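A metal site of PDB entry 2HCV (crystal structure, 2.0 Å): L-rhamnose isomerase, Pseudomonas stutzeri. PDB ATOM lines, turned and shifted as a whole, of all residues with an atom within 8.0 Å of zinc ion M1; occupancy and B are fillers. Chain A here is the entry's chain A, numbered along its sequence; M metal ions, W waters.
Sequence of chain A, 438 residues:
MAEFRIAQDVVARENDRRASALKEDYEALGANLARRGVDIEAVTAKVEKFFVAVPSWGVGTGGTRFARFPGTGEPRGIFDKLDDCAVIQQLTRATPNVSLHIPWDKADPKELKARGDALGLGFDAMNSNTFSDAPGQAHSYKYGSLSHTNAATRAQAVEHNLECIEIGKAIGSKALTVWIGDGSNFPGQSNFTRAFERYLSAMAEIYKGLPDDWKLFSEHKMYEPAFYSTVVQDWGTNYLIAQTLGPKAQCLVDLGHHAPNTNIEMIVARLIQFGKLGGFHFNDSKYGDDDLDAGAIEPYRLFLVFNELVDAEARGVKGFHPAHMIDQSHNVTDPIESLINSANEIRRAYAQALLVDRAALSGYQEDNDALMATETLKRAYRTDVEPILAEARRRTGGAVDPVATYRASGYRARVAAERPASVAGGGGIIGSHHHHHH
O of Asp 327 is in hydrogen-bond range of ND2 of Asn 283 (2.9 Å). The backbone carbonyl oxygen (O) of His 281 sits at hydrogen-bond distance from the backbone NH (N) of Leu 255 (3.2 Å). The backbone carbonyl oxygen (O) of Val 253 sits at hydrogen-bond distance from the backbone NH (N) of His 281 (2.8 Å). OD1 of Asp 254 is in hydrogen-bond range of ND2 of Asn 283. N of Asp 327 is in hydrogen-bond range of O of Phe 282, at 3.0 Å. OD1 of Asp 327 lies within hydrogen-bond range of NE1 of Trp 57, at 3.3 Å. The side-chain carboxylate (OD1) of Asp 254 sits at hydrogen-bond distance from the backbone NH (N) of Gly 256, at 3.3 Å.
Zinc ion M1 is bound by OD2 of Asp 327, OE2 of Glu 219, OD2 of Asp 254, water W2 and ND1 of His 281. Zinc ion M1 has five donor atoms within binding distance. Slightly farther from zinc ion M1 lies water W1 (2.7 Å).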
ATOM      1  N   TRP A  57     -16.578 -24.252 -24.447  1.00  0.00           N
ATOM      2  CA  TRP A  57     -16.253 -22.912 -24.912  1.00  0.00           C
ATOM      3  C   TRP A  57     -16.636 -21.833 -23.903  1.00  0.00           C
ATOM      4  O   TRP A  57     -16.391 -20.650 -24.119  1.00  0.00           O
ATOM      5  CB  TRP A  57     -16.943 -22.647 -26.254  1.00  0.00           C
ATOM      6  CG  TRP A  57     -18.450 -22.681 -26.215  1.00  0.00           C
ATOM      7  CD1 TRP A  57     -19.276 -21.604 -26.093  1.00  0.00           C
ATOM      8  CD2 TRP A  57     -19.296 -23.836 -26.303  1.00  0.00           C
ATOM      9  NE1 TRP A  57     -20.590 -22.009 -26.091  1.00  0.00           N
ATOM     10  CE2 TRP A  57     -20.624 -23.378 -26.222  1.00  0.00           C
ATOM     11  CE3 TRP A  57     -19.053 -25.206 -26.440  1.00  0.00           C
ATOM     12  CZ2 TRP A  57     -21.725 -24.243 -26.274  1.00  0.00           C
ATOM     13  CZ3 TRP A  57     -20.140 -26.070 -26.489  1.00  0.00           C
ATOM     14  CH2 TRP A  57     -21.461 -25.584 -26.408  1.00  0.00           C
ATOM     15  N   ASN A 127     -21.426 -30.396 -30.554  1.00  0.00           N
ATOM     16  CA  ASN A 127     -21.843 -29.150 -31.192  1.00  0.00           C
ATOM     17  C   ASN A 127     -21.013 -28.928 -32.454  1.00  0.00           C
ATOM     18  O   ASN A 127     -19.791 -28.832 -32.392  1.00  0.00           O
ATOM     19  CB  ASN A 127     -21.638 -27.976 -30.233  1.00  0.00           C
ATOM     20  CG  ASN A 127     -22.614 -28.007 -29.085  1.00  0.00           C
ATOM     21  OD1 ASN A 127     -23.717 -27.468 -29.177  1.00  0.00           O
ATOM     22  ND2 ASN A 127     -22.221 -28.662 -27.989  1.00  0.00           N
ATOM     23  N   THR A 177     -25.999 -31.198 -31.522  1.00  0.00           N
ATOM     24  CA  THR A 177     -26.749 -29.958 -31.566  1.00  0.00           C
ATOM     25  C   THR A 177     -26.256 -29.152 -32.760  1.00  0.00           C
ATOM     26  O   THR A 177     -25.050 -28.959 -32.933  1.00  0.00           O
ATOM     27  CB  THR A 177     -26.554 -29.121 -30.290  1.00  0.00           C
ATOM     28  OG1 THR A 177     -27.135 -29.807 -29.176  1.00  0.00           O
ATOM     29  CG2 THR A 177     -27.219 -27.753 -30.441  1.00  0.00           C
ATOM     30  N   TRP A 179     -26.574 -25.543 -34.582  1.00  0.00           N
ATOM     31  CA  TRP A 179     -26.976 -24.141 -34.613  1.00  0.00           C
ATOM     32  C   TRP A 179     -26.094 -23.515 -35.675  1.00  0.00           C
ATOM     33  O   TRP A 179     -24.869 -23.634 -35.598  1.00  0.00           O
ATOM     34  CB  TRP A 179     -26.744 -23.414 -33.296  1.00  0.00           C
ATOM     35  CG  TRP A 179     -26.943 -21.918 -33.473  1.00  0.00           C
ATOM     36  CD1 TRP A 179     -28.146 -21.258 -33.588  1.00  0.00           C
ATOM     37  CD2 TRP A 179     -25.928 -20.943 -33.735  1.00  0.00           C
ATOM     38  NE1 TRP A 179     -27.932 -19.937 -33.907  1.00  0.00           N
ATOM     39  CE2 TRP A 179     -26.579 -19.717 -33.997  1.00  0.00           C
ATOM     40  CE3 TRP A 179     -24.523 -20.983 -33.763  1.00  0.00           C
ATOM     41  CZ2 TRP A 179     -25.874 -18.536 -34.293  1.00  0.00           C
ATOM     42  CZ3 TRP A 179     -23.826 -19.807 -34.056  1.00  0.00           C
ATOM     43  CH2 TRP A 179     -24.504 -18.598 -34.320  1.00  0.00           C
ATOM     44  N   GLU A 219     -31.417 -25.778 -33.279  1.00  0.00           N
ATOM     45  CA  GLU A 219     -31.568 -24.645 -32.379  1.00  0.00           C
ATOM     46  C   GLU A 219     -31.940 -23.363 -33.122  1.00  0.00           C
ATOM     47  O   GLU A 219     -31.156 -22.873 -33.919  1.00  0.00           O
ATOM     48  CB  GLU A 219     -30.262 -24.423 -31.627  1.00  0.00           C
ATOM     49  CG  GLU A 219     -30.292 -23.330 -30.576  1.00  0.00           C
ATOM     50  CD  GLU A 219     -28.940 -23.155 -29.897  1.00  0.00           C
ATOM     51  OE1 GLU A 219     -28.120 -24.093 -29.948  1.00  0.00           O
ATOM     52  OE2 GLU A 219     -28.718 -22.090 -29.300  1.00  0.00           O
ATOM     53  N   HIS A 220     -33.125 -22.831 -32.844  1.00  0.00           N
ATOM     54  CA  HIS A 220     -33.569 -21.610 -33.521  1.00  0.00           C
ATOM     55  C   HIS A 220     -32.984 -20.348 -32.886  1.00  0.00           C
ATOM     56  O   HIS A 220     -32.566 -20.351 -31.724  1.00  0.00           O
ATOM     57  CB  HIS A 220     -35.107 -21.521 -33.520  1.00  0.00           C
ATOM     58  CG  HIS A 220     -35.725 -21.542 -32.157  1.00  0.00           C
ATOM     59  ND1 HIS A 220     -36.097 -22.710 -31.531  1.00  0.00           N
ATOM     60  CD2 HIS A 220     -36.009 -20.544 -31.291  1.00  0.00           C
ATOM     61  CE1 HIS A 220     -36.600 -22.434 -30.336  1.00  0.00           C
ATOM     62  NE2 HIS A 220     -36.557 -21.117 -30.174  1.00  0.00           N
ATOM     63  N   LYS A 221     -32.958 -19.267 -33.669  1.00  0.00           N
ATOM     64  CA  LYS A 221     -32.445 -17.993 -33.203  1.00  0.00           C
ATOM     65  C   LYS A 221     -33.036 -16.909 -34.113  1.00  0.00           C
ATOM     66  O   LYS A 221     -32.967 -17.000 -35.337  1.00  0.00           O
ATOM     67  CB  LYS A 221     -30.910 -17.967 -33.272  1.00  0.00           C
ATOM     68  CG  LYS A 221     -30.273 -16.763 -32.603  1.00  0.00           C
ATOM     69  CD  LYS A 221     -28.752 -16.872 -32.556  1.00  0.00           C
ATOM     70  CE  LYS A 221     -28.130 -15.644 -31.888  1.00  0.00           C
ATOM     71  NZ  LYS A 221     -26.642 -15.723 -31.791  1.00  0.00           N
ATOM     72  N   LEU A 252     -34.207 -27.517 -29.690  1.00  0.00           N
ATOM     73  CA  LEU A 252     -33.473 -27.027 -28.545  1.00  0.00           C
ATOM     74  C   LEU A 252     -33.854 -25.560 -28.354  1.00  0.00           C
ATOM     75  O   LEU A 252     -33.847 -24.776 -29.311  1.00  0.00           O
ATOM     76  CB  LEU A 252     -31.981 -27.181 -28.790  1.00  0.00           C
ATOM     77  CG  LEU A 252     -31.027 -26.853 -27.636  1.00  0.00           C
ATOM     78  CD1 LEU A 252     -29.751 -27.670 -27.799  1.00  0.00           C
ATOM     79  CD2 LEU A 252     -30.736 -25.363 -27.606  1.00  0.00           C
ATOM     80  N   VAL A 253     -34.207 -25.196 -27.127  1.00  0.00           N
ATOM     81  CA  VAL A 253     -34.599 -23.818 -26.807  1.00  0.00           C
ATOM     82  C   VAL A 253     -33.506 -23.071 -26.045  1.00  0.00           C
ATOM     83  O   VAL A 253     -33.145 -23.462 -24.934  1.00  0.00           O
ATOM     84  CB  VAL A 253     -35.894 -23.786 -25.964  1.00  0.00           C
ATOM     85  CG1 VAL A 253     -36.331 -22.346 -25.711  1.00  0.00           C
ATOM     86  CG2 VAL A 253     -37.005 -24.546 -26.672  1.00  0.00           C
ATOM     87  N   ASP A 254     -32.998 -22.001 -26.648  1.00  0.00           N
ATOM     88  CA  ASP A 254     -31.973 -21.179 -26.017  1.00  0.00           C
ATOM     89  C   ASP A 254     -32.690 -19.906 -25.554  1.00  0.00           C
ATOM     90  O   ASP A 254     -33.208 -19.144 -26.360  1.00  0.00           O
ATOM     91  CB  ASP A 254     -30.870 -20.824 -27.024  1.00  0.00           C
ATOM     92  CG  ASP A 254     -29.722 -20.050 -26.384  1.00  0.00           C
ATOM     93  OD1 ASP A 254     -29.994 -19.079 -25.668  1.00  0.00           O
ATOM     94  OD2 ASP A 254     -28.546 -20.413 -26.611  1.00  0.00           O
ATOM     95  N   LEU A 255     -32.725 -19.700 -24.237  1.00  0.00           N
ATOM     96  CA  LEU A 255     -33.411 -18.557 -23.637  1.00  0.00           C
ATOM     97  C   LEU A 255     -33.297 -17.193 -24.334  1.00  0.00           C
ATOM     98  O   LEU A 255     -34.309 -16.530 -24.557  1.00  0.00           O
ATOM     99  CB  LEU A 255     -32.991 -18.389 -22.178  1.00  0.00           C
ATOM    100  CG  LEU A 255     -33.780 -19.207 -21.151  1.00  0.00           C
ATOM    101  CD1 LEU A 255     -33.135 -19.098 -19.783  1.00  0.00           C
ATOM    102  CD2 LEU A 255     -35.217 -18.702 -21.105  1.00  0.00           C
ATOM    103  N   GLY A 256     -32.085 -16.779 -24.662  1.00  0.00           N
ATOM    104  CA  GLY A 256     -31.897 -15.477 -25.286  1.00  0.00           C
ATOM    105  C   GLY A 256     -32.081 -15.396 -26.798  1.00  0.00           C
ATOM    106  O   GLY A 256     -31.730 -14.383 -27.407  1.00  0.00           O
ATOM    107  N   HIS A 257     -32.650 -16.439 -27.401  1.00  0.00           N
ATOM    108  CA  HIS A 257     -32.861 -16.449 -28.848  1.00  0.00           C
ATOM    109  C   HIS A 257     -34.254 -16.045 -29.317  1.00  0.00           C
ATOM    110  O   HIS A 257     -34.657 -16.376 -30.435  1.00  0.00           O
ATOM    111  CB  HIS A 257     -32.566 -17.848 -29.411  1.00  0.00           C
ATOM    112  CG  HIS A 257     -31.103 -18.194 -29.432  1.00  0.00           C
ATOM    113  ND1 HIS A 257     -30.606 -19.241 -30.174  1.00  0.00           N
ATOM    114  CD2 HIS A 257     -30.038 -17.632 -28.819  1.00  0.00           C
ATOM    115  CE1 HIS A 257     -29.296 -19.306 -30.030  1.00  0.00           C
ATOM    116  NE2 HIS A 257     -28.924 -18.337 -29.211  1.00  0.00           N
ATOM    117  N   PHE A 280     -32.559 -27.624 -23.536  1.00  0.00           N
ATOM    118  CA  PHE A 280     -32.646 -26.213 -23.223  1.00  0.00           C
ATOM    119  C   PHE A 280     -31.277 -25.628 -22.941  1.00  0.00           C
ATOM    120  O   PHE A 280     -30.515 -26.161 -22.118  1.00  0.00           O
ATOM    121  CB  PHE A 280     -33.571 -26.036 -22.007  1.00  0.00           C
ATOM    122  CG  PHE A 280     -34.165 -24.662 -21.886  1.00  0.00           C
ATOM    123  CD1 PHE A 280     -33.442 -23.614 -21.326  1.00  0.00           C
ATOM    124  CD2 PHE A 280     -35.454 -24.401 -22.352  1.00  0.00           C
ATOM    125  CE1 PHE A 280     -33.977 -22.336 -21.235  1.00  0.00           C
ATOM    126  CE2 PHE A 280     -36.008 -23.120 -22.270  1.00  0.00           C
ATOM    127  CZ  PHE A 280     -35.269 -22.079 -21.714  1.00  0.00           C
ATOM    128  N   HIS A 281     -30.936 -24.547 -23.644  1.00  0.00           N
ATOM    129  CA  HIS A 281     -29.661 -23.864 -23.435  1.00  0.00           C
ATOM    130  C   HIS A 281     -29.953 -22.712 -22.485  1.00  0.00           C
ATOM    131  O   HIS A 281     -30.689 -21.782 -22.816  1.00  0.00           O
ATOM    132  CB  HIS A 281     -29.105 -23.305 -24.748  1.00  0.00           C
ATOM    133  CG  HIS A 281     -28.309 -24.297 -25.538  1.00  0.00           C
ATOM    134  ND1 HIS A 281     -27.588 -23.940 -26.658  1.00  0.00           N
ATOM    135  CD2 HIS A 281     -28.118 -25.631 -25.378  1.00  0.00           C
ATOM    136  CE1 HIS A 281     -26.992 -25.006 -27.155  1.00  0.00           C
ATOM    137  NE2 HIS A 281     -27.296 -26.047 -26.397  1.00  0.00           N
ATOM    138  N   PHE A 282     -29.374 -22.787 -21.292  1.00  0.00           N
ATOM    139  CA  PHE A 282     -29.573 -21.776 -20.252  1.00  0.00           C
ATOM    140  C   PHE A 282     -28.627 -20.575 -20.297  1.00  0.00           C
ATOM    141  O   PHE A 282     -27.431 -20.707 -20.579  1.00  0.00           O
ATOM    142  CB  PHE A 282     -29.489 -22.440 -18.873  1.00  0.00           C
ATOM    143  CG  PHE A 282     -30.601 -23.410 -18.596  1.00  0.00           C
ATOM    144  CD1 PHE A 282     -31.865 -22.952 -18.209  1.00  0.00           C
ATOM    145  CD2 PHE A 282     -30.405 -24.777 -18.748  1.00  0.00           C
ATOM    146  CE1 PHE A 282     -32.900 -23.848 -17.965  1.00  0.00           C
ATOM    147  CE2 PHE A 282     -31.439 -25.680 -18.511  1.00  0.00           C
ATOM    148  CZ  PHE A 282     -32.683 -25.210 -18.118  1.00  0.00           C
ATOM    149  N   ASN A 283     -29.198 -19.411 -20.025  1.00  0.00           N
ATOM    150  CA  ASN A 283     -28.493 -18.136 -19.970  1.00  0.00           C
ATOM    151  C   ASN A 283     -29.537 -17.071 -19.677  1.00  0.00           C
ATOM    152  O   ASN A 283     -30.727 -17.371 -19.562  1.00  0.00           O
ATOM    153  CB  ASN A 283     -27.775 -17.826 -21.299  1.00  0.00           C
ATOM    154  CG  ASN A 283     -28.688 -17.935 -22.504  1.00  0.00           C
ATOM    155  OD1 ASN A 283     -29.733 -17.275 -22.580  1.00  0.00           O
ATOM    156  ND2 ASN A 283     -28.292 -18.763 -23.473  1.00  0.00           N
ATOM    157  N   ASP A 289     -29.438 -11.620 -27.649  1.00  0.00           N
ATOM    158  CA  ASP A 289     -28.842 -12.888 -27.232  1.00  0.00           C
ATOM    159  C   ASP A 289     -27.568 -12.520 -26.486  1.00  0.00           C
ATOM    160  O   ASP A 289     -26.459 -12.767 -26.950  1.00  0.00           O
ATOM    161  CB  ASP A 289     -28.520 -13.757 -28.447  1.00  0.00           C
ATOM    162  CG  ASP A 289     -27.857 -15.058 -28.067  1.00  0.00           C
ATOM    163  OD1 ASP A 289     -28.241 -15.653 -27.037  1.00  0.00           O
ATOM    164  OD2 ASP A 289     -26.951 -15.502 -28.804  1.00  0.00           O
ATOM    165  N   ASP A 291     -26.330 -13.716 -23.759  1.00  0.00           N
ATOM    166  CA  ASP A 291     -25.590 -14.841 -23.191  1.00  0.00           C
ATOM    167  C   ASP A 291     -25.013 -14.549 -21.801  1.00  0.00           C
ATOM    168  O   ASP A 291     -23.894 -14.944 -21.503  1.00  0.00           O
ATOM    169  CB  ASP A 291     -24.432 -15.245 -24.123  1.00  0.00           C
ATOM    170  CG  ASP A 291     -24.913 -15.877 -25.411  1.00  0.00           C
ATOM    171  OD1 ASP A 291     -25.888 -16.661 -25.354  1.00  0.00           O
ATOM    172  OD2 ASP A 291     -24.316 -15.625 -26.476  1.00  0.00           O
ATOM    173  N   MET A 325     -28.276 -27.704 -20.839  1.00  0.00           N
ATOM    174  CA  MET A 325     -26.930 -27.223 -21.058  1.00  0.00           C
ATOM    175  C   MET A 325     -26.822 -25.721 -20.858  1.00  0.00           C
ATOM    176  O   MET A 325     -27.752 -24.974 -21.171  1.00  0.00           O
ATOM    177  CB  MET A 325     -26.477 -27.583 -22.477  1.00  0.00           C
ATOM    178  CG  MET A 325     -26.639 -29.069 -22.799  1.00  0.00           C
ATOM    179  SD  MET A 325     -26.670 -29.445 -24.552  1.00  0.00           S
ATOM    180  CE  MET A 325     -28.428 -29.488 -24.854  1.00  0.00           C
ATOM    181  N   ILE A 326     -25.690 -25.285 -20.330  1.00  0.00           N
ATOM    182  CA  ILE A 326     -25.446 -23.866 -20.141  1.00  0.00           C
ATOM    183  C   ILE A 326     -24.771 -23.356 -21.400  1.00  0.00           C
ATOM    184  O   ILE A 326     -23.803 -23.944 -21.868  1.00  0.00           O
ATOM    185  CB  ILE A 326     -24.491 -23.613 -18.949  1.00  0.00           C
ATOM    186  CG1 ILE A 326     -25.127 -24.072 -17.646  1.00  0.00           C
ATOM    187  CG2 ILE A 326     -24.121 -22.122 -18.885  1.00  0.00           C
ATOM    188  CD1 ILE A 326     -24.224 -23.926 -16.437  1.00  0.00           C
ATOM    189  N   ASP A 327     -25.296 -22.279 -21.982  1.00  0.00           N
ATOM    190  CA  ASP A 327     -24.683 -21.698 -23.167  1.00  0.00           C
ATOM    191  C   ASP A 327     -24.545 -20.212 -22.897  1.00  0.00           C
ATOM    192  O   ASP A 327     -25.468 -19.434 -23.151  1.00  0.00           O
ATOM    193  CB  ASP A 327     -25.532 -21.936 -24.411  1.00  0.00           C
ATOM    194  CG  ASP A 327     -24.855 -21.433 -25.677  1.00  0.00           C
ATOM    195  OD1 ASP A 327     -23.680 -21.015 -25.607  1.00  0.00           O
ATOM    196  OD2 ASP A 327     -25.488 -21.465 -26.747  1.00  0.00           O
ATOM    197  N   GLN A 328     -23.391 -19.829 -22.366  1.00  0.00           N
ATOM    198  CA  GLN A 328     -23.133 -18.449 -22.006  1.00  0.00           C
ATOM    199  C   GLN A 328     -21.767 -17.948 -22.486  1.00  0.00           C
ATOM    200  O   GLN A 328     -20.936 -18.714 -22.971  1.00  0.00           O
ATOM    201  CB  GLN A 328     -23.226 -18.287 -20.487  1.00  0.00           C
ATOM    202  CG  GLN A 328     -24.575 -18.693 -19.897  1.00  0.00           C
ATOM    203  CD  GLN A 328     -24.575 -18.757 -18.375  1.00  0.00           C
ATOM    204  OE1 GLN A 328     -25.628 -19.001 -17.771  1.00  0.00           O
ATOM    205  NE2 GLN A 328     -23.421 -18.549 -17.753  1.00  0.00           N
HETATM  206 ZN    ZN M   1     -27.246 -21.874 -27.722  1.00  0.00          ZN
HETATM  207 ZN    ZN M   2     -26.805 -18.107 -29.163  1.00  0.00          ZN
HETATM  208  O   HOH W   1     -25.532 -22.637 -29.653  1.00  0.00           O
HETATM  209  O   HOH W   2     -26.383 -20.234 -29.091  1.00  0.00           O
